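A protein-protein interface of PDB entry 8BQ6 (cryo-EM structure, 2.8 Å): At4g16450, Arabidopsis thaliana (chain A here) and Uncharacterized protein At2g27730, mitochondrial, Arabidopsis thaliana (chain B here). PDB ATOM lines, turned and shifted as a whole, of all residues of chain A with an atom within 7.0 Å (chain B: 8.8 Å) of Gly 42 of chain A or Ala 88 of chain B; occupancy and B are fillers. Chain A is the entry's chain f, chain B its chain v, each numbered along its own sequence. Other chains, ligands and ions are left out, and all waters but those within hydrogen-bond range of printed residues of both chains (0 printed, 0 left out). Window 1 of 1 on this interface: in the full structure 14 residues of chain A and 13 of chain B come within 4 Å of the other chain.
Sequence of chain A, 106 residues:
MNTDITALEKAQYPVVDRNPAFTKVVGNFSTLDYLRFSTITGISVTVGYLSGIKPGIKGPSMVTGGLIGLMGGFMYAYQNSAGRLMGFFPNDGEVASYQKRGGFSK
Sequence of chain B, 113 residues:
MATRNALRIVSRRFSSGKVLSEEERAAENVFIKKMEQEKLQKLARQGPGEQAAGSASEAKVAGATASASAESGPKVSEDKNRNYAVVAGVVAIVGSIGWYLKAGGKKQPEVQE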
ATOM      1  N   ARG A  36     -12.029   9.212 -12.236  1.00  0.00           N
ATOM      2  CA  ARG A  36     -10.881   8.609 -12.913  1.00  0.00           C
ATOM      3  C   ARG A  36      -9.898   9.676 -13.375  1.00  0.00           C
ATOM      4  O   ARG A  36      -8.679   9.556 -13.178  1.00  0.00           O
ATOM      5  CB  ARG A  36     -11.341   7.786 -14.116  1.00  0.00           C
ATOM      6  CG  ARG A  36     -12.252   6.634 -13.803  1.00  0.00           C
ATOM      7  CD  ARG A  36     -13.055   6.269 -15.033  1.00  0.00           C
ATOM      8  NE  ARG A  36     -13.703   4.971 -14.889  1.00  0.00           N
ATOM      9  CZ  ARG A  36     -14.917   4.688 -15.335  1.00  0.00           C
ATOM     10  NH1 ARG A  36     -15.649   5.591 -15.966  1.00  0.00           N
ATOM     11  NH2 ARG A  36     -15.409   3.467 -15.145  1.00  0.00           N
ATOM     12  N   PHE A  37     -10.424  10.723 -14.011  1.00  0.00           N
ATOM     13  CA  PHE A  37      -9.602  11.834 -14.471  1.00  0.00           C
ATOM     14  C   PHE A  37      -8.779  12.421 -13.329  1.00  0.00           C
ATOM     15  O   PHE A  37      -7.549  12.550 -13.426  1.00  0.00           O
ATOM     16  CB  PHE A  37     -10.526  12.886 -15.082  1.00  0.00           C
ATOM     17  CG  PHE A  37      -9.843  13.862 -15.968  1.00  0.00           C
ATOM     18  CD1 PHE A  37      -8.472  13.859 -16.109  1.00  0.00           C
ATOM     19  CD2 PHE A  37     -10.578  14.793 -16.669  1.00  0.00           C
ATOM     20  CE1 PHE A  37      -7.852  14.765 -16.920  1.00  0.00           C
ATOM     21  CE2 PHE A  37      -9.960  15.696 -17.484  1.00  0.00           C
ATOM     22  CZ  PHE A  37      -8.593  15.683 -17.608  1.00  0.00           C
ATOM     23  N   SER A  38      -9.448  12.765 -12.229  1.00  0.00           N
ATOM     24  CA  SER A  38      -8.778  13.395 -11.102  1.00  0.00           C
ATOM     25  C   SER A  38      -7.773  12.458 -10.448  1.00  0.00           C
ATOM     26  O   SER A  38      -6.691  12.896 -10.049  1.00  0.00           O
ATOM     27  CB  SER A  38      -9.814  13.877 -10.090  1.00  0.00           C
ATOM     28  OG  SER A  38     -10.862  14.574 -10.742  1.00  0.00           O
ATOM     29  N   THR A  39      -8.104  11.171 -10.315  1.00  0.00           N
ATOM     30  CA  THR A  39      -7.160  10.243  -9.703  1.00  0.00           C
ATOM     31  C   THR A  39      -5.885  10.135 -10.530  1.00  0.00           C
ATOM     32  O   THR A  39      -4.772  10.214  -9.990  1.00  0.00           O
ATOM     33  CB  THR A  39      -7.808   8.870  -9.516  1.00  0.00           C
ATOM     34  OG1 THR A  39      -8.838   8.963  -8.527  1.00  0.00           O
ATOM     35  CG2 THR A  39      -6.785   7.848  -9.067  1.00  0.00           C
ATOM     36  N   ILE A  40      -6.026   9.975 -11.850  1.00  0.00           N
ATOM     37  CA  ILE A  40      -4.839   9.846 -12.693  1.00  0.00           C
ATOM     38  C   ILE A  40      -4.001  11.116 -12.627  1.00  0.00           C
ATOM     39  O   ILE A  40      -2.773  11.063 -12.462  1.00  0.00           O
ATOM     40  CB  ILE A  40      -5.242   9.496 -14.138  1.00  0.00           C
ATOM     41  CG1 ILE A  40      -5.784   8.072 -14.193  1.00  0.00           C
ATOM     42  CG2 ILE A  40      -4.053   9.622 -15.079  1.00  0.00           C
ATOM     43  CD1 ILE A  40      -6.785   7.852 -15.294  1.00  0.00           C
ATOM     44  N   THR A  41      -4.653  12.277 -12.718  1.00  0.00           N
ATOM     45  CA  THR A  41      -3.915  13.536 -12.681  1.00  0.00           C
ATOM     46  C   THR A  41      -3.200  13.737 -11.345  1.00  0.00           C
ATOM     47  O   THR A  41      -2.037  14.158 -11.318  1.00  0.00           O
ATOM     48  CB  THR A  41      -4.863  14.695 -12.977  1.00  0.00           C
ATOM     49  OG1 THR A  41      -5.520  14.458 -14.229  1.00  0.00           O
ATOM     50  CG2 THR A  41      -4.108  16.013 -13.035  1.00  0.00           C
ATOM     51  N   GLY A  42      -3.871  13.436 -10.231  1.00  0.00           N
ATOM     52  CA  GLY A  42      -3.250  13.624  -8.928  1.00  0.00           C
ATOM     53  C   GLY A  42      -2.075  12.693  -8.692  1.00  0.00           C
ATOM     54  O   GLY A  42      -1.030  13.112  -8.178  1.00  0.00           O
ATOM     55  N   ILE A  43      -2.220  11.422  -9.076  1.00  0.00           N
ATOM     56  CA  ILE A  43      -1.103  10.487  -8.974  1.00  0.00           C
ATOM     57  C   ILE A  43       0.070  10.968  -9.817  1.00  0.00           C
ATOM     58  O   ILE A  43       1.235  10.852  -9.414  1.00  0.00           O
ATOM     59  CB  ILE A  43      -1.544   9.074  -9.394  1.00  0.00           C
ATOM     60  CG1 ILE A  43      -2.458   8.459  -8.340  1.00  0.00           C
ATOM     61  CG2 ILE A  43      -0.342   8.179  -9.633  1.00  0.00           C
ATOM     62  CD1 ILE A  43      -3.133   7.203  -8.820  1.00  0.00           C
ATOM     63  N   SER A  44      -0.214  11.493 -11.006  1.00  0.00           N
ATOM     64  CA  SER A  44       0.865  11.905 -11.894  1.00  0.00           C
ATOM     65  C   SER A  44       1.594  13.131 -11.357  1.00  0.00           C
ATOM     66  O   SER A  44       2.829  13.202 -11.418  1.00  0.00           O
ATOM     67  CB  SER A  44       0.294  12.168 -13.278  1.00  0.00           C
ATOM     68  OG  SER A  44      -0.114  10.951 -13.871  1.00  0.00           O
ATOM     69  N   VAL A  45       0.850  14.098 -10.823  1.00  0.00           N
ATOM     70  CA  VAL A  45       1.474  15.251 -10.179  1.00  0.00           C
ATOM     71  C   VAL A  45       2.351  14.795  -9.019  1.00  0.00           C
ATOM     72  O   VAL A  45       3.476  15.284  -8.837  1.00  0.00           O
ATOM     73  CB  VAL A  45       0.394  16.249  -9.724  1.00  0.00           C
ATOM     74  CG1 VAL A  45       1.003  17.391  -8.969  1.00  0.00           C
ATOM     75  CG2 VAL A  45      -0.367  16.780 -10.916  1.00  0.00           C
ATOM     76  N   THR A  46       1.855  13.843  -8.223  1.00  0.00           N
ATOM     77  CA  THR A  46       2.609  13.365  -7.069  1.00  0.00           C
ATOM     78  C   THR A  46       3.900  12.668  -7.484  1.00  0.00           C
ATOM     79  O   THR A  46       4.956  12.884  -6.876  1.00  0.00           O
ATOM     80  CB  THR A  46       1.732  12.426  -6.245  1.00  0.00           C
ATOM     81  OG1 THR A  46       0.731  13.192  -5.567  1.00  0.00           O
ATOM     82  CG2 THR A  46       2.557  11.667  -5.225  1.00  0.00           C
ATOM     83  N   VAL A  47       3.831  11.809  -8.504  1.00  0.00           N
ATOM     84  CA  VAL A  47       5.032  11.131  -8.979  1.00  0.00           C
ATOM     85  C   VAL A  47       6.025  12.148  -9.524  1.00  0.00           C
ATOM     86  O   VAL A  47       7.237  12.045  -9.288  1.00  0.00           O
ATOM     87  CB  VAL A  47       4.674  10.060 -10.028  1.00  0.00           C
ATOM     88  CG1 VAL A  47       5.920   9.566 -10.741  1.00  0.00           C
ATOM     89  CG2 VAL A  47       3.949   8.900  -9.375  1.00  0.00           C
ATOM     90  N   GLY A  48       5.528  13.155 -10.247  1.00  0.00           N
ATOM     91  CA  GLY A  48       6.410  14.206 -10.728  1.00  0.00           C
ATOM     92  C   GLY A  48       7.122  14.924  -9.600  1.00  0.00           C
ATOM     93  O   GLY A  48       8.330  15.161  -9.662  1.00  0.00           O
ATOM     94  N   MET A  62       6.866  18.406 -11.331  1.00  0.00           N
ATOM     95  CA  MET A  62       5.451  18.333 -10.995  1.00  0.00           C
ATOM     96  C   MET A  62       4.589  18.748 -12.177  1.00  0.00           C
ATOM     97  O   MET A  62       3.572  18.113 -12.469  1.00  0.00           O
ATOM     98  CB  MET A  62       5.173  19.220  -9.786  1.00  0.00           C
ATOM     99  CG  MET A  62       3.994  18.788  -8.976  1.00  0.00           C
ATOM    100  SD  MET A  62       3.840  19.603  -7.380  1.00  0.00           S
ATOM    101  CE  MET A  62       4.753  21.106  -7.686  1.00  0.00           C
ATOM    102  N   GLY A  66       2.148  16.320 -14.196  1.00  0.00           N
ATOM    103  CA  GLY A  66       0.754  16.716 -14.279  1.00  0.00           C
ATOM    104  C   GLY A  66       0.243  16.787 -15.703  1.00  0.00           C
ATOM    105  O   GLY A  66      -0.916  16.476 -15.962  1.00  0.00           O
ATOM    106  N   GLY A  69      -0.283  13.220 -16.807  1.00  0.00           N
ATOM    107  CA  GLY A  69      -1.497  12.736 -16.175  1.00  0.00           C
ATOM    108  C   GLY A  69      -2.762  13.362 -16.729  1.00  0.00           C
ATOM    109  O   GLY A  69      -3.791  12.698 -16.830  1.00  0.00           O
ATOM    110  N   ASN B  81       5.308  24.653  -3.636  1.00  0.00           N
ATOM    111  CA  ASN B  81       5.325  23.431  -4.435  1.00  0.00           C
ATOM    112  C   ASN B  81       5.040  22.217  -3.565  1.00  0.00           C
ATOM    113  O   ASN B  81       4.325  21.297  -3.979  1.00  0.00           O
ATOM    114  CB  ASN B  81       6.667  23.277  -5.150  1.00  0.00           C
ATOM    115  CG  ASN B  81       6.804  24.210  -6.334  1.00  0.00           C
ATOM    116  OD1 ASN B  81       5.823  24.773  -6.816  1.00  0.00           O
ATOM    117  ND2 ASN B  81       8.027  24.369  -6.818  1.00  0.00           N
ATOM    118  N   ARG B  82       5.568  22.214  -2.341  1.00  0.00           N
ATOM    119  CA  ARG B  82       5.229  21.156  -1.399  1.00  0.00           C
ATOM    120  C   ARG B  82       3.734  21.141  -1.102  1.00  0.00           C
ATOM    121  O   ARG B  82       3.119  20.071  -1.047  1.00  0.00           O
ATOM    122  CB  ARG B  82       6.036  21.322  -0.114  1.00  0.00           C
ATOM    123  CG  ARG B  82       5.964  20.118   0.803  1.00  0.00           C
ATOM    124  CD  ARG B  82       6.831  20.301   2.029  1.00  0.00           C
ATOM    125  NE  ARG B  82       6.376  21.412   2.854  1.00  0.00           N
ATOM    126  CZ  ARG B  82       7.165  22.372   3.316  1.00  0.00           C
ATOM    127  NH1 ARG B  82       8.457  22.400   3.034  1.00  0.00           N
ATOM    128  NH2 ARG B  82       6.644  23.327   4.079  1.00  0.00           N
ATOM    129  N   ASN B  83       3.126  22.317  -0.918  1.00  0.00           N
ATOM    130  CA  ASN B  83       1.692  22.364  -0.634  1.00  0.00           C
ATOM    131  C   ASN B  83       0.867  21.852  -1.808  1.00  0.00           C
ATOM    132  O   ASN B  83      -0.113  21.121  -1.614  1.00  0.00           O
ATOM    133  CB  ASN B  83       1.269  23.782  -0.257  1.00  0.00           C
ATOM    134  CG  ASN B  83       2.035  24.315   0.924  1.00  0.00           C
ATOM    135  OD1 ASN B  83       2.471  23.549   1.782  1.00  0.00           O
ATOM    136  ND2 ASN B  83       2.157  25.630   1.012  1.00  0.00           N
ATOM    137  N   TYR B  84       1.240  22.228  -3.030  1.00  0.00           N
ATOM    138  CA  TYR B  84       0.531  21.732  -4.205  1.00  0.00           C
ATOM    139  C   TYR B  84       0.683  20.226  -4.337  1.00  0.00           C
ATOM    140  O   TYR B  84      -0.265  19.528  -4.714  1.00  0.00           O
ATOM    141  CB  TYR B  84       1.043  22.428  -5.464  1.00  0.00           C
ATOM    142  CG  TYR B  84       0.890  23.924  -5.437  1.00  0.00           C
ATOM    143  CD1 TYR B  84      -0.093  24.526  -4.670  1.00  0.00           C
ATOM    144  CD2 TYR B  84       1.737  24.736  -6.171  1.00  0.00           C
ATOM    145  CE1 TYR B  84      -0.232  25.892  -4.639  1.00  0.00           C
ATOM    146  CE2 TYR B  84       1.606  26.103  -6.149  1.00  0.00           C
ATOM    147  CZ  TYR B  84       0.619  26.676  -5.380  1.00  0.00           C
ATOM    148  OH  TYR B  84       0.484  28.042  -5.352  1.00  0.00           O
ATOM    149  N   ALA B  85       1.874  19.705  -4.035  1.00  0.00           N
ATOM    150  CA  ALA B  85       2.070  18.260  -4.059  1.00  0.00           C
ATOM    151  C   ALA B  85       1.198  17.571  -3.023  1.00  0.00           C
ATOM    152  O   ALA B  85       0.639  16.499  -3.279  1.00  0.00           O
ATOM    153  CB  ALA B  85       3.540  17.929  -3.825  1.00  0.00           C
ATOM    154  N   VAL B  86       1.084  18.168  -1.838  1.00  0.00           N
ATOM    155  CA  VAL B  86       0.222  17.617  -0.797  1.00  0.00           C
ATOM    156  C   VAL B  86      -1.226  17.586  -1.271  1.00  0.00           C
ATOM    157  O   VAL B  86      -1.943  16.596  -1.075  1.00  0.00           O
ATOM    158  CB  VAL B  86       0.382  18.434   0.497  1.00  0.00           C
ATOM    159  CG1 VAL B  86      -0.745  18.152   1.444  1.00  0.00           C
ATOM    160  CG2 VAL B  86       1.721  18.143   1.148  1.00  0.00           C
ATOM    161  N   VAL B  87      -1.674  18.673  -1.903  1.00  0.00           N
ATOM    162  CA  VAL B  87      -3.034  18.724  -2.431  1.00  0.00           C
ATOM    163  C   VAL B  87      -3.235  17.642  -3.480  1.00  0.00           C
ATOM    164  O   VAL B  87      -4.280  16.986  -3.521  1.00  0.00           O
ATOM    165  CB  VAL B  87      -3.339  20.121  -2.999  1.00  0.00           C
ATOM    166  CG1 VAL B  87      -4.687  20.129  -3.695  1.00  0.00           C
ATOM    167  CG2 VAL B  87      -3.299  21.159  -1.905  1.00  0.00           C
ATOM    168  N   ALA B  88      -2.246  17.451  -4.354  1.00  0.00           N
ATOM    169  CA  ALA B  88      -2.346  16.415  -5.379  1.00  0.00           C
ATOM    170  C   ALA B  88      -2.435  15.027  -4.763  1.00  0.00           C
ATOM    171  O   ALA B  88      -3.210  14.184  -5.225  1.00  0.00           O
ATOM    172  CB  ALA B  88      -1.150  16.494  -6.322  1.00  0.00           C
ATOM    173  N   GLY B  89      -1.635  14.763  -3.731  1.00  0.00           N
ATOM    174  CA  GLY B  89      -1.703  13.469  -3.072  1.00  0.00           C
ATOM    175  C   GLY B  89      -3.044  13.230  -2.403  1.00  0.00           C
ATOM    176  O   GLY B  89      -3.609  12.134  -2.490  1.00  0.00           O
ATOM    177  N   VAL B  90      -3.579  14.255  -1.739  1.00  0.00           N
ATOM    178  CA  VAL B  90      -4.892  14.129  -1.115  1.00  0.00           C
ATOM    179  C   VAL B  90      -5.966  13.920  -2.174  1.00  0.00           C
ATOM    180  O   VAL B  90      -6.883  13.106  -2.001  1.00  0.00           O
ATOM    181  CB  VAL B  90      -5.188  15.363  -0.245  1.00  0.00           C
ATOM    182  CG1 VAL B  90      -6.675  15.483   0.030  1.00  0.00           C
ATOM    183  CG2 VAL B  90      -4.410  15.285   1.048  1.00  0.00           C
ATOM    184  N   VAL B  91      -5.880  14.664  -3.277  1.00  0.00           N
ATOM    185  CA  VAL B  91      -6.846  14.523  -4.358  1.00  0.00           C
ATOM    186  C   VAL B  91      -6.796  13.114  -4.922  1.00  0.00           C
ATOM    187  O   VAL B  91      -7.833  12.501  -5.179  1.00  0.00           O
ATOM    188  CB  VAL B  91      -6.595  15.583  -5.446  1.00  0.00           C
ATOM    189  CG1 VAL B  91      -7.109  15.104  -6.794  1.00  0.00           C
ATOM    190  CG2 VAL B  91      -7.252  16.891  -5.062  1.00  0.00           C
ATOM    191  N   ALA B  92      -5.592  12.572  -5.100  1.00  0.00           N
ATOM    192  CA  ALA B  92      -5.463  11.207  -5.595  1.00  0.00           C
ATOM    193  C   ALA B  92      -6.072  10.204  -4.621  1.00  0.00           C
ATOM    194  O   ALA B  92      -6.752   9.262  -5.038  1.00  0.00           O
ATOM    195  CB  ALA B  92      -3.995  10.882  -5.865  1.00  0.00           C
ATOM    196  N   ILE B  93      -5.850  10.389  -3.316  1.00  0.00           N
ATOM    197  CA  ILE B  93      -6.385   9.423  -2.353  1.00  0.00           C
ATOM    198  C   ILE B  93      -7.912   9.481  -2.321  1.00  0.00           C
ATOM    199  O   ILE B  93      -8.594   8.450  -2.417  1.00  0.00           O
ATOM    200  CB  ILE B  93      -5.781   9.649  -0.955  1.00  0.00           C
ATOM    201  CG1 ILE B  93      -4.360   9.088  -0.896  1.00  0.00           C
ATOM    202  CG2 ILE B  93      -6.623   8.950   0.095  1.00  0.00           C
ATOM    203  CD1 ILE B  93      -3.451   9.807   0.070  1.00  0.00           C
ATOM    204  N   VAL B  94      -8.471  10.687  -2.198  1.00  0.00           N
ATOM    205  CA  VAL B  94      -9.925  10.834  -2.155  1.00  0.00           C
ATOM    206  C   VAL B  94     -10.546  10.368  -3.466  1.00  0.00           C
ATOM    207  O   VAL B  94     -11.622   9.760  -3.478  1.00  0.00           O
ATOM    208  CB  VAL B  94     -10.313  12.290  -1.835  1.00  0.00           C
ATOM    209  CG1 VAL B  94     -11.832  12.466  -1.865  1.00  0.00           C
ATOM    210  CG2 VAL B  94      -9.744  12.719  -0.495  1.00  0.00           C
ATOM    211  N   GLY B  95      -9.880  10.644  -4.590  1.00  0.00           N
ATOM    212  CA  GLY B  95     -10.393  10.208  -5.873  1.00  0.00           C
ATOM    213  C   GLY B  95     -10.362   8.704  -6.043  1.00  0.00           C
ATOM    214  O   GLY B  95     -11.290   8.125  -6.604  1.00  0.00           O
ATOM    215  N   SER B  96      -9.297   8.047  -5.573  1.00  0.00           N
ATOM    216  CA  SER B  96      -9.278   6.586  -5.603  1.00  0.00           C
ATOM    217  C   SER B  96     -10.386   6.009  -4.735  1.00  0.00           C
ATOM    218  O   SER B  96     -11.034   5.022  -5.116  1.00  0.00           O
ATOM    219  CB  SER B  96      -7.919   6.050  -5.150  1.00  0.00           C
ATOM    220  OG  SER B  96      -6.845   6.676  -5.828  1.00  0.00           O
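The side-chain hydroxyl (OG1) of Thr 39 of chain A lies close to the backbone carbonyl oxygen (O) of Gly 95 of chain B (3.2 Å).
The side-chain hydroxyl of Thr 39 of chain A sits at hydrogen-bond distance from the backbone NH of Ser 96 of chain B, at 3.1 Å.
The backbone NH (N) of Gly 89 of chain B is in hydrogen-bond range of the side-chain hydroxyl (OG1) of Thr 46 of chain A, at 3.4 Å.
The side-chain hydroxyl (OG1) of Thr 46 of chain A sits at hydrogen-bond distance from the backbone carbonyl oxygen (O) of Gly 42 of chain A (3.2 Å).
The backbone carbonyl oxygen of Ala 92 of chain B sits at hydrogen-bond distance from the side-chain hydroxyl of Ser 96 of chain B, 2.7 Å away.
Among the printed residues, merely in contact across the chains: Val 45 of chain A with Ala 88 of chain B, Ile 43 of chain A with Ala 92 of chain B, Met 62 of chain A with Asn 81 of chain B, Gly 42 of chain A with Ala 88 of chain B, Thr 46 of chain A with Ala 88 of chain B, Gly 42 of chain A with Ala 92 of chain B, Met 62 of chain A with Ala 85 of chain B and Ser 38 of chain A with Val 91 of chain B.
No residue of chain B comes within 4 Å of Thr 41 of chain A.
Gly 42 of chain A touches two residues of chain B.
Printed residues of chain A within 4 Å of Asn 81 of chain B: Met 62 (3.7 Å).
Ala 88 of chain B touches just these residues of chain A: Gly 42, Val 45 and Thr 46.
Printed residues of chain A within 4 Å of Gly 89 of chain B: Thr 46 (3.4 Å).
Val 90 of chain B touches none of the printed residues of chain A.
Printed residues of chain A within 4 Å of Gly 95 of chain B: Thr 39.
Printed residues of chain A within 4 Å of Ser 96 of chain B: Thr 39 (3.1 Å).
The nearest residue of chain A that does not touch Ala 88 of chain B is Ile 43 of chain A (4.8 Å).
The nearest printed residue of chain A that does not touch Ser 96 of chain B is Ile 43 of chain A (4.8 Å).
Among the printed residues, 11 pairs touch across the chains.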
